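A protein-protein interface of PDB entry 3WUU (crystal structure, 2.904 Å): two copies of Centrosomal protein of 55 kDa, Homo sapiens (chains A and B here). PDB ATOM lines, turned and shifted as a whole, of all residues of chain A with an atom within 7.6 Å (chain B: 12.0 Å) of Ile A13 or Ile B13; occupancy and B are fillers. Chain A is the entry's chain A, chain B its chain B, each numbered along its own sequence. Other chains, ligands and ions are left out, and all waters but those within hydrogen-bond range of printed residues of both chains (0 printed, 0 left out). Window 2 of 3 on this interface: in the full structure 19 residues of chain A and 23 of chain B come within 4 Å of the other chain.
Printed residues of chain B that touch a printed residue of chain A: Ile B13, Met B16, Glu B17 and Leu B20. Hydrophobic or aromatic side chains of chain B that line the printed part of chain A: Ile B13, Met B16 and Leu B20. Hydrophobic or aromatic side chains of chain A within 4 Å of the printed part of chain B: Ile A13 and Met A16. Along chain A the printed residues that touch a printed residue of chain B span positions 13 to 19. Among the printed residues, 7 pairs touch across the chains.
Ile A13 touches its own counterpart, Ile B13. Ile A13 touches Met B16, but with the chains exchanged Met A16 does not touch Ile B13 (4.5 Å). Met B16 touches its own counterpart, Met A16. Met A16 touches Glu B17, and with the chains exchanged Glu A17 touches Met B16. Of the 7 pairs that touch across the chains among the printed residues, 4 have their exchanged pair printed and touching as well.
No residue of chain B comes within 4 Å of Ser A9. Ile A10 touches none of the printed residues of chain B. No residue of chain B comes within 4 Å of Asn A12. Ile A13 touches just these residues of chain B: Ile B13 (3.5 Å) and Met B16 (3.8 Å). His A14 touches none of the printed residues of chain B. Of chain B, only Met B16 (3.7 Å), Glu B17 (3.9 Å) and Leu B20 (3.96 Å) come within 4 Å of Met A16. Glu A17 touches just one residue of chain B: Met B16. Ser B5 touches none of the printed residues of chain A. Ile B13 touches just one residue of chain A: Ile A13. Of the printed residues of chain A, Glu B17 touches Met A16 (3.9 Å). Printed residues of chain A within 4 Å of Leu B20: Met A16 and Gln A19. Lys B21 touches none of the printed residues of chain A. The nearest residue of chain A that does not touch Ile B13 is Met A16 (4.5 Å). The nearest printed residue of chain A that does not touch Met B16 is His A14 (6.0 Å).
Ile B13 touches Ile A13 (CG2 to CG1, 3.5 Å). Met B16 touches Ile A13. CG of Met A16 touches CE of Met B16, at 3.7 Å. Glu B17 touches Met A16 (CA to SD, 3.9 Å). Met A16 touches Leu B20 (O to CD2, 3.96 Å). Met B16 touches Glu A17 (SD to CA, 3.8 Å). Leu B20 touches Gln A19.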
ATOM      1  N   SER A   8     -14.776 -29.541   8.521  1.00  0.00           N
ATOM      2  CA  SER A   8     -14.695 -30.402   9.694  1.00  0.00           C
ATOM      3  C   SER A   8     -15.774 -30.041  10.706  1.00  0.00           C
ATOM      4  O   SER A   8     -16.429 -30.917  11.273  1.00  0.00           O
ATOM      5  CB  SER A   8     -13.319 -30.286  10.348  1.00  0.00           C
ATOM      6  OG  SER A   8     -13.147 -29.009  10.940  1.00  0.00           O
ATOM      7  N   SER A   9     -15.957 -28.742  10.923  1.00  0.00           N
ATOM      8  CA  SER A   9     -16.921 -28.247  11.899  1.00  0.00           C
ATOM      9  C   SER A   9     -18.355 -28.611  11.527  1.00  0.00           C
ATOM     10  O   SER A   9     -19.234 -28.659  12.387  1.00  0.00           O
ATOM     11  CB  SER A   9     -16.780 -26.734  12.069  1.00  0.00           C
ATOM     12  OG  SER A   9     -15.493 -26.400  12.562  1.00  0.00           O
ATOM     13  N   ILE A  10     -18.585 -28.865  10.244  1.00  0.00           N
ATOM     14  CA  ILE A  10     -19.887 -29.316   9.770  1.00  0.00           C
ATOM     15  C   ILE A  10     -20.150 -30.762  10.205  1.00  0.00           C
ATOM     16  O   ILE A  10     -21.272 -31.114  10.581  1.00  0.00           O
ATOM     17  CB  ILE A  10     -20.004 -29.170   8.233  1.00  0.00           C
ATOM     18  CG1 ILE A  10     -20.455 -27.753   7.872  1.00  0.00           C
ATOM     19  CG2 ILE A  10     -20.966 -30.195   7.647  1.00  0.00           C
ATOM     20  CD1 ILE A  10     -20.675 -27.535   6.388  1.00  0.00           C
ATOM     21  N   ASN A  11     -19.107 -31.589  10.180  1.00  0.00           N
ATOM     22  CA  ASN A  11     -19.236 -33.006  10.526  1.00  0.00           C
ATOM     23  C   ASN A  11     -19.542 -33.294  12.003  1.00  0.00           C
ATOM     24  O   ASN A  11     -20.175 -34.301  12.317  1.00  0.00           O
ATOM     25  CB  ASN A  11     -17.987 -33.781  10.082  1.00  0.00           C
ATOM     26  CG  ASN A  11     -17.942 -34.015   8.583  1.00  0.00           C
ATOM     27  OD1 ASN A  11     -18.971 -34.015   7.908  1.00  0.00           O
ATOM     28  ND2 ASN A  11     -16.739 -34.224   8.057  1.00  0.00           N
ATOM     29  N   ASN A  12     -19.073 -32.422  12.893  1.00  0.00           N
ATOM     30  CA  ASN A  12     -19.379 -32.510  14.314  1.00  0.00           C
ATOM     31  C   ASN A  12     -20.875 -32.376  14.516  1.00  0.00           C
ATOM     32  O   ASN A  12     -21.507 -33.154  15.236  1.00  0.00           O
ATOM     33  CB  ASN A  12     -18.720 -31.357  15.064  1.00  0.00           C
ATOM     34  CG  ASN A  12     -17.237 -31.534  15.256  1.00  0.00           C
ATOM     35  OD1 ASN A  12     -16.589 -32.311  14.563  1.00  0.00           O
ATOM     36  ND2 ASN A  12     -16.683 -30.794  16.217  1.00  0.00           N
ATOM     37  N   ILE A  13     -21.409 -31.346  13.869  1.00  0.00           N
ATOM     38  CA  ILE A  13     -22.828 -31.029  13.865  1.00  0.00           C
ATOM     39  C   ILE A  13     -23.673 -32.226  13.395  1.00  0.00           C
ATOM     40  O   ILE A  13     -24.830 -32.374  13.788  1.00  0.00           O
ATOM     41  CB  ILE A  13     -23.080 -29.705  13.053  1.00  0.00           C
ATOM     42  CG1 ILE A  13     -23.131 -28.487  13.989  1.00  0.00           C
ATOM     43  CG2 ILE A  13     -24.283 -29.812  12.102  1.00  0.00           C
ATOM     44  CD1 ILE A  13     -21.786 -27.787  14.188  1.00  0.00           C
ATOM     45  N   HIS A  14     -23.070 -33.093  12.585  1.00  0.00           N
ATOM     46  CA  HIS A  14     -23.666 -34.384  12.238  1.00  0.00           C
ATOM     47  C   HIS A  14     -23.596 -35.357  13.422  1.00  0.00           C
ATOM     48  O   HIS A  14     -24.544 -36.097  13.684  1.00  0.00           O
ATOM     49  CB  HIS A  14     -22.978 -35.011  11.019  1.00  0.00           C
ATOM     50  CG  HIS A  14     -23.558 -34.596   9.702  1.00  0.00           C
ATOM     51  ND1 HIS A  14     -24.762 -35.076   9.238  1.00  0.00           N
ATOM     52  CD2 HIS A  14     -23.081 -33.776   8.736  1.00  0.00           C
ATOM     53  CE1 HIS A  14     -25.013 -34.554   8.048  1.00  0.00           C
ATOM     54  NE2 HIS A  14     -24.008 -33.764   7.723  1.00  0.00           N
ATOM     55  N   GLU A  15     -22.463 -35.362  14.123  1.00  0.00           N
ATOM     56  CA  GLU A  15     -22.278 -36.197  15.315  1.00  0.00           C
ATOM     57  C   GLU A  15     -23.168 -35.735  16.468  1.00  0.00           C
ATOM     58  O   GLU A  15     -23.670 -36.548  17.245  1.00  0.00           O
ATOM     59  CB  GLU A  15     -20.811 -36.171  15.760  1.00  0.00           C
ATOM     60  CG  GLU A  15     -19.884 -37.003  14.893  1.00  0.00           C
ATOM     61  CD  GLU A  15     -20.282 -38.469  14.865  1.00  0.00           C
ATOM     62  OE1 GLU A  15     -20.716 -38.992  15.914  1.00  0.00           O
ATOM     63  OE2 GLU A  15     -20.167 -39.098  13.791  1.00  0.00           O
ATOM     64  N   MET A  16     -23.340 -34.420  16.568  1.00  0.00           N
ATOM     65  CA  MET A  16     -24.176 -33.782  17.581  1.00  0.00           C
ATOM     66  C   MET A  16     -25.608 -34.266  17.510  1.00  0.00           C
ATOM     67  O   MET A  16     -26.247 -34.519  18.533  1.00  0.00           O
ATOM     68  CB  MET A  16     -24.171 -32.273  17.371  1.00  0.00           C
ATOM     69  CG  MET A  16     -25.212 -31.530  18.183  1.00  0.00           C
ATOM     70  SD  MET A  16     -24.630 -29.881  18.592  1.00  0.00           S
ATOM     71  CE  MET A  16     -23.164 -30.331  19.504  1.00  0.00           C
ATOM     72  N   GLU A  17     -26.114 -34.356  16.285  1.00  0.00           N
ATOM     73  CA  GLU A  17     -27.470 -34.821  16.051  1.00  0.00           C
ATOM     74  C   GLU A  17     -27.562 -36.262  16.534  1.00  0.00           C
ATOM     75  O   GLU A  17     -28.510 -36.637  17.223  1.00  0.00           O
ATOM     76  CB  GLU A  17     -27.834 -34.728  14.565  1.00  0.00           C
ATOM     77  CG  GLU A  17     -29.329 -34.590  14.308  1.00  0.00           C
ATOM     78  CD  GLU A  17     -29.761 -35.091  12.940  1.00  0.00           C
ATOM     79  OE1 GLU A  17     -28.890 -35.343  12.080  1.00  0.00           O
ATOM     80  OE2 GLU A  17     -30.985 -35.238  12.732  1.00  0.00           O
ATOM     81  N   ILE A  18     -26.550 -37.054  16.192  1.00  0.00           N
ATOM     82  CA  ILE A  18     -26.472 -38.454  16.591  1.00  0.00           C
ATOM     83  C   ILE A  18     -26.452 -38.588  18.111  1.00  0.00           C
ATOM     84  O   ILE A  18     -27.110 -39.464  18.679  1.00  0.00           O
ATOM     85  CB  ILE A  18     -25.198 -39.110  16.004  1.00  0.00           C
ATOM     86  CG1 ILE A  18     -25.312 -39.212  14.483  1.00  0.00           C
ATOM     87  CG2 ILE A  18     -24.959 -40.481  16.617  1.00  0.00           C
ATOM     88  CD1 ILE A  18     -24.125 -39.880  13.824  1.00  0.00           C
ATOM     89  N   GLN A  19     -25.696 -37.705  18.754  1.00  0.00           N
ATOM     90  CA  GLN A  19     -25.562 -37.702  20.203  1.00  0.00           C
ATOM     91  C   GLN A  19     -26.864 -37.314  20.881  1.00  0.00           C
ATOM     92  O   GLN A  19     -27.244 -37.916  21.880  1.00  0.00           O
ATOM     93  CB  GLN A  19     -24.456 -36.741  20.638  1.00  0.00           C
ATOM     94  CG  GLN A  19     -23.045 -37.205  20.351  1.00  0.00           C
ATOM     95  CD  GLN A  19     -22.686 -38.476  21.088  1.00  0.00           C
ATOM     96  OE1 GLN A  19     -22.712 -39.564  20.517  1.00  0.00           O
ATOM     97  NE2 GLN A  19     -22.346 -38.346  22.366  1.00  0.00           N
ATOM     98  N   SER B   5     -33.751 -19.153   5.884  1.00  0.00           N
ATOM     99  CA  SER B   5     -32.454 -18.483   5.892  1.00  0.00           C
ATOM    100  C   SER B   5     -31.418 -19.249   6.715  1.00  0.00           C
ATOM    101  O   SER B   5     -31.766 -20.007   7.623  1.00  0.00           O
ATOM    102  CB  SER B   5     -32.595 -17.049   6.410  1.00  0.00           C
ATOM    103  OG  SER B   5     -33.241 -17.026   7.669  1.00  0.00           O
ATOM    104  N   PHE B   6     -30.146 -19.042   6.385  1.00  0.00           N
ATOM    105  CA  PHE B   6     -29.039 -19.712   7.059  1.00  0.00           C
ATOM    106  C   PHE B   6     -28.945 -19.324   8.536  1.00  0.00           C
ATOM    107  O   PHE B   6     -28.699 -20.175   9.393  1.00  0.00           O
ATOM    108  CB  PHE B   6     -27.715 -19.398   6.346  1.00  0.00           C
ATOM    109  CG  PHE B   6     -27.618 -19.961   4.949  1.00  0.00           C
ATOM    110  CD1 PHE B   6     -28.154 -21.204   4.639  1.00  0.00           C
ATOM    111  CD2 PHE B   6     -26.984 -19.245   3.944  1.00  0.00           C
ATOM    112  CE1 PHE B   6     -28.060 -21.718   3.353  1.00  0.00           C
ATOM    113  CE2 PHE B   6     -26.888 -19.754   2.657  1.00  0.00           C
ATOM    114  CZ  PHE B   6     -27.425 -20.991   2.363  1.00  0.00           C
ATOM    115  N   ASN B   7     -29.142 -18.040   8.828  1.00  0.00           N
ATOM    116  CA  ASN B   7     -29.122 -17.545  10.204  1.00  0.00           C
ATOM    117  C   ASN B   7     -30.231 -18.175  11.042  1.00  0.00           C
ATOM    118  O   ASN B   7     -30.135 -18.257  12.269  1.00  0.00           O
ATOM    119  CB  ASN B   7     -29.248 -16.019  10.223  1.00  0.00           C
ATOM    120  CG  ASN B   7     -29.001 -15.426  11.598  1.00  0.00           C
ATOM    121  OD1 ASN B   7     -29.933 -14.993  12.278  1.00  0.00           O
ATOM    122  ND2 ASN B   7     -27.739 -15.403  12.015  1.00  0.00           N
ATOM    123  N   SER B   8     -31.286 -18.616  10.365  1.00  0.00           N
ATOM    124  CA  SER B   8     -32.356 -19.369  11.001  1.00  0.00           C
ATOM    125  C   SER B   8     -31.915 -20.803  11.282  1.00  0.00           C
ATOM    126  O   SER B   8     -32.347 -21.410  12.261  1.00  0.00           O
ATOM    127  CB  SER B   8     -33.607 -19.368  10.121  1.00  0.00           C
ATOM    128  OG  SER B   8     -34.435 -20.478  10.413  1.00  0.00           O
ATOM    129  N   SER B   9     -31.051 -21.339  10.422  1.00  0.00           N
ATOM    130  CA  SER B   9     -30.564 -22.707  10.580  1.00  0.00           C
ATOM    131  C   SER B   9     -29.460 -22.799  11.625  1.00  0.00           C
ATOM    132  O   SER B   9     -29.343 -23.800  12.328  1.00  0.00           O
ATOM    133  CB  SER B   9     -30.066 -23.263   9.248  1.00  0.00           C
ATOM    134  OG  SER B   9     -31.128 -23.355   8.318  1.00  0.00           O
ATOM    135  N   ILE B  10     -28.649 -21.752  11.713  1.00  0.00           N
ATOM    136  CA  ILE B  10     -27.600 -21.686  12.719  1.00  0.00           C
ATOM    137  C   ILE B  10     -28.224 -21.556  14.106  1.00  0.00           C
ATOM    138  O   ILE B  10     -27.690 -22.065  15.091  1.00  0.00           O
ATOM    139  CB  ILE B  10     -26.630 -20.522  12.442  1.00  0.00           C
ATOM    140  CG1 ILE B  10     -25.972 -20.709  11.074  1.00  0.00           C
ATOM    141  CG2 ILE B  10     -25.568 -20.422  13.527  1.00  0.00           C
ATOM    142  CD1 ILE B  10     -24.882 -19.710  10.774  1.00  0.00           C
ATOM    143  N   ASN B  11     -29.373 -20.890  14.173  1.00  0.00           N
ATOM    144  CA  ASN B  11     -30.113 -20.780  15.424  1.00  0.00           C
ATOM    145  C   ASN B  11     -30.618 -22.133  15.920  1.00  0.00           C
ATOM    146  O   ASN B  11     -30.654 -22.386  17.124  1.00  0.00           O
ATOM    147  CB  ASN B  11     -31.275 -19.796  15.288  1.00  0.00           C
ATOM    148  CG  ASN B  11     -30.974 -18.455  15.922  1.00  0.00           C
ATOM    149  OD1 ASN B  11     -29.813 -18.107  16.136  1.00  0.00           O
ATOM    150  ND2 ASN B  11     -32.020 -17.699  16.234  1.00  0.00           N
ATOM    151  N   ASN B  12     -31.008 -22.996  14.987  1.00  0.00           N
ATOM    152  CA  ASN B  12     -31.451 -24.343  15.329  1.00  0.00           C
ATOM    153  C   ASN B  12     -30.312 -25.189  15.885  1.00  0.00           C
ATOM    154  O   ASN B  12     -30.489 -25.922  16.858  1.00  0.00           O
ATOM    155  CB  ASN B  12     -32.071 -25.037  14.115  1.00  0.00           C
ATOM    156  CG  ASN B  12     -33.312 -24.329  13.613  1.00  0.00           C
ATOM    157  OD1 ASN B  12     -33.904 -23.513  14.320  1.00  0.00           O
ATOM    158  ND2 ASN B  12     -33.716 -24.642  12.387  1.00  0.00           N
ATOM    159  N   ILE B  13     -29.145 -25.082  15.256  1.00  0.00           N
ATOM    160  CA  ILE B  13     -27.958 -25.794  15.709  1.00  0.00           C
ATOM    161  C   ILE B  13     -27.584 -25.370  17.127  1.00  0.00           C
ATOM    162  O   ILE B  13     -27.159 -26.193  17.942  1.00  0.00           O
ATOM    163  CB  ILE B  13     -26.766 -25.554  14.766  1.00  0.00           C
ATOM    164  CG1 ILE B  13     -27.143 -25.890  13.321  1.00  0.00           C
ATOM    165  CG2 ILE B  13     -25.569 -26.358  15.214  1.00  0.00           C
ATOM    166  CD1 ILE B  13     -27.748 -27.263  13.141  1.00  0.00           C
ATOM    167  N   HIS B  14     -27.752 -24.082  17.417  1.00  0.00           N
ATOM    168  CA  HIS B  14     -27.565 -23.557  18.767  1.00  0.00           C
ATOM    169  C   HIS B  14     -28.559 -24.203  19.735  1.00  0.00           C
ATOM    170  O   HIS B  14     -28.203 -24.546  20.862  1.00  0.00           O
ATOM    171  CB  HIS B  14     -27.737 -22.033  18.777  1.00  0.00           C
ATOM    172  CG  HIS B  14     -26.454 -21.277  18.929  1.00  0.00           C
ATOM    173  ND1 HIS B  14     -25.729 -20.813  17.850  1.00  0.00           N
ATOM    174  CD2 HIS B  14     -25.767 -20.898  20.032  1.00  0.00           C
ATOM    175  CE1 HIS B  14     -24.652 -20.185  18.284  1.00  0.00           C
ATOM    176  NE2 HIS B  14     -24.650 -20.223  19.606  1.00  0.00           N
ATOM    177  N   GLU B  15     -29.801 -24.362  19.280  1.00  0.00           N
ATOM    178  CA  GLU B  15     -30.849 -25.000  20.073  1.00  0.00           C
ATOM    179  C   GLU B  15     -30.556 -26.480  20.276  1.00  0.00           C
ATOM    180  O   GLU B  15     -30.728 -27.015  21.372  1.00  0.00           O
ATOM    181  CB  GLU B  15     -32.216 -24.820  19.403  1.00  0.00           C
ATOM    182  CG  GLU B  15     -33.380 -25.455  20.161  1.00  0.00           C
ATOM    183  CD  GLU B  15     -33.740 -24.692  21.423  1.00  0.00           C
ATOM    184  OE1 GLU B  15     -33.769 -23.444  21.376  1.00  0.00           O
ATOM    185  OE2 GLU B  15     -33.994 -25.342  22.461  1.00  0.00           O
ATOM    186  N   MET B  16     -30.115 -27.137  19.207  1.00  0.00           N
ATOM    187  CA  MET B  16     -29.734 -28.545  19.266  1.00  0.00           C
ATOM    188  C   MET B  16     -28.639 -28.774  20.307  1.00  0.00           C
ATOM    189  O   MET B  16     -28.660 -29.762  21.044  1.00  0.00           O
ATOM    190  CB  MET B  16     -29.261 -29.037  17.893  1.00  0.00           C
ATOM    191  CG  MET B  16     -28.785 -30.481  17.882  1.00  0.00           C
ATOM    192  SD  MET B  16     -28.527 -31.153  16.224  1.00  0.00           S
ATOM    193  CE  MET B  16     -27.293 -30.027  15.581  1.00  0.00           C
ATOM    194  N   GLU B  17     -27.689 -27.847  20.369  1.00  0.00           N
ATOM    195  CA  GLU B  17     -26.614 -27.927  21.343  1.00  0.00           C
ATOM    196  C   GLU B  17     -27.161 -27.774  22.755  1.00  0.00           C
ATOM    197  O   GLU B  17     -26.707 -28.448  23.680  1.00  0.00           O
ATOM    198  CB  GLU B  17     -25.561 -26.852  21.079  1.00  0.00           C
ATOM    199  CG  GLU B  17     -24.387 -26.903  22.045  1.00  0.00           C
ATOM    200  CD  GLU B  17     -23.750 -25.545  22.266  1.00  0.00           C
ATOM    201  OE1 GLU B  17     -24.302 -24.539  21.773  1.00  0.00           O
ATOM    202  OE2 GLU B  17     -22.699 -25.483  22.939  1.00  0.00           O
ATOM    203  N   ILE B  18     -28.132 -26.879  22.918  1.00  0.00           N
ATOM    204  CA  ILE B  18     -28.763 -26.667  24.216  1.00  0.00           C
ATOM    205  C   ILE B  18     -29.466 -27.939  24.666  1.00  0.00           C
ATOM    206  O   ILE B  18     -29.377 -28.332  25.828  1.00  0.00           O
ATOM    207  CB  ILE B  18     -29.786 -25.516  24.179  1.00  0.00           C
ATOM    208  CG1 ILE B  18     -29.097 -24.194  23.834  1.00  0.00           C
ATOM    209  CG2 ILE B  18     -30.510 -25.400  25.512  1.00  0.00           C
ATOM    210  CD1 ILE B  18     -27.978 -23.820  24.777  1.00  0.00           C
ATOM    211  N   GLN B  19     -30.152 -28.584  23.729  1.00  0.00           N
ATOM    212  CA  GLN B  19     -30.887 -29.804  24.025  1.00  0.00           C
ATOM    213  C   GLN B  19     -29.961 -30.966  24.371  1.00  0.00           C
ATOM    214  O   GLN B  19     -30.313 -31.823  25.180  1.00  0.00           O
ATOM    215  CB  GLN B  19     -31.796 -30.184  22.853  1.00  0.00           C
ATOM    216  CG  GLN B  19     -32.935 -29.210  22.610  1.00  0.00           C
ATOM    217  CD  GLN B  19     -33.836 -29.646  21.472  1.00  0.00           C
ATOM    218  OE1 GLN B  19     -33.557 -30.633  20.788  1.00  0.00           O
ATOM    219  NE2 GLN B  19     -34.925 -28.915  21.266  1.00  0.00           N
ATOM    220  N   LEU B  20     -28.778 -30.995  23.762  1.00  0.00           N
ATOM    221  CA  LEU B  20     -27.826 -32.073  24.024  1.00  0.00           C
ATOM    222  C   LEU B  20     -27.183 -31.919  25.397  1.00  0.00           C
ATOM    223  O   LEU B  20     -27.038 -32.894  26.133  1.00  0.00           O
ATOM    224  CB  LEU B  20     -26.747 -32.145  22.940  1.00  0.00           C
ATOM    225  CG  LEU B  20     -25.732 -33.277  23.146  1.00  0.00           C
ATOM    226  CD1 LEU B  20     -26.442 -34.610  23.319  1.00  0.00           C
ATOM    227  CD2 LEU B  20     -24.739 -33.353  21.999  1.00  0.00           C
ATOM    228  N   LYS B  21     -26.806 -30.689  25.733  1.00  0.00           N
ATOM    229  CA  LYS B  21     -26.239 -30.385  27.042  1.00  0.00           C
ATOM    230  C   LYS B  21     -27.246 -30.738  28.125  1.00  0.00           C
ATOM    231  O   LYS B  21     -26.882 -31.051  29.260  1.00  0.00           O
ATOM    232  CB  LYS B  21     -25.870 -28.904  27.124  1.00  0.00           C
ATOM    233  CG  LYS B  21     -25.158 -28.500  28.406  1.00  0.00           C
ATOM    234  CD  LYS B  21     -24.766 -27.033  28.367  1.00  0.00           C
ATOM    235  CE  LYS B  21     -23.869 -26.730  27.173  1.00  0.00           C
ATOM    236  NZ  LYS B  21     -23.548 -25.275  27.069  1.00  0.00           N
ATOM    237  N   ASP B  22     -28.520 -30.692  27.753  1.00  0.00           N
ATOM    238  CA  ASP B  22     -29.607 -31.024  28.656  1.00  0.00           C
ATOM    239  C   ASP B  22     -29.806 -32.535  28.734  1.00  0.00           C
ATOM    240  O   ASP B  22     -29.907 -33.098  29.821  1.00  0.00           O
ATOM    241  CB  ASP B  22     -30.889 -30.337  28.188  1.00  0.00           C
ATOM    242  CG  ASP B  22     -32.068 -30.624  29.091  1.00  0.00           C
ATOM    243  OD1 ASP B  22     -32.064 -30.141  30.243  1.00  0.00           O
ATOM    244  OD2 ASP B  22     -33.001 -31.326  28.645  1.00  0.00           O
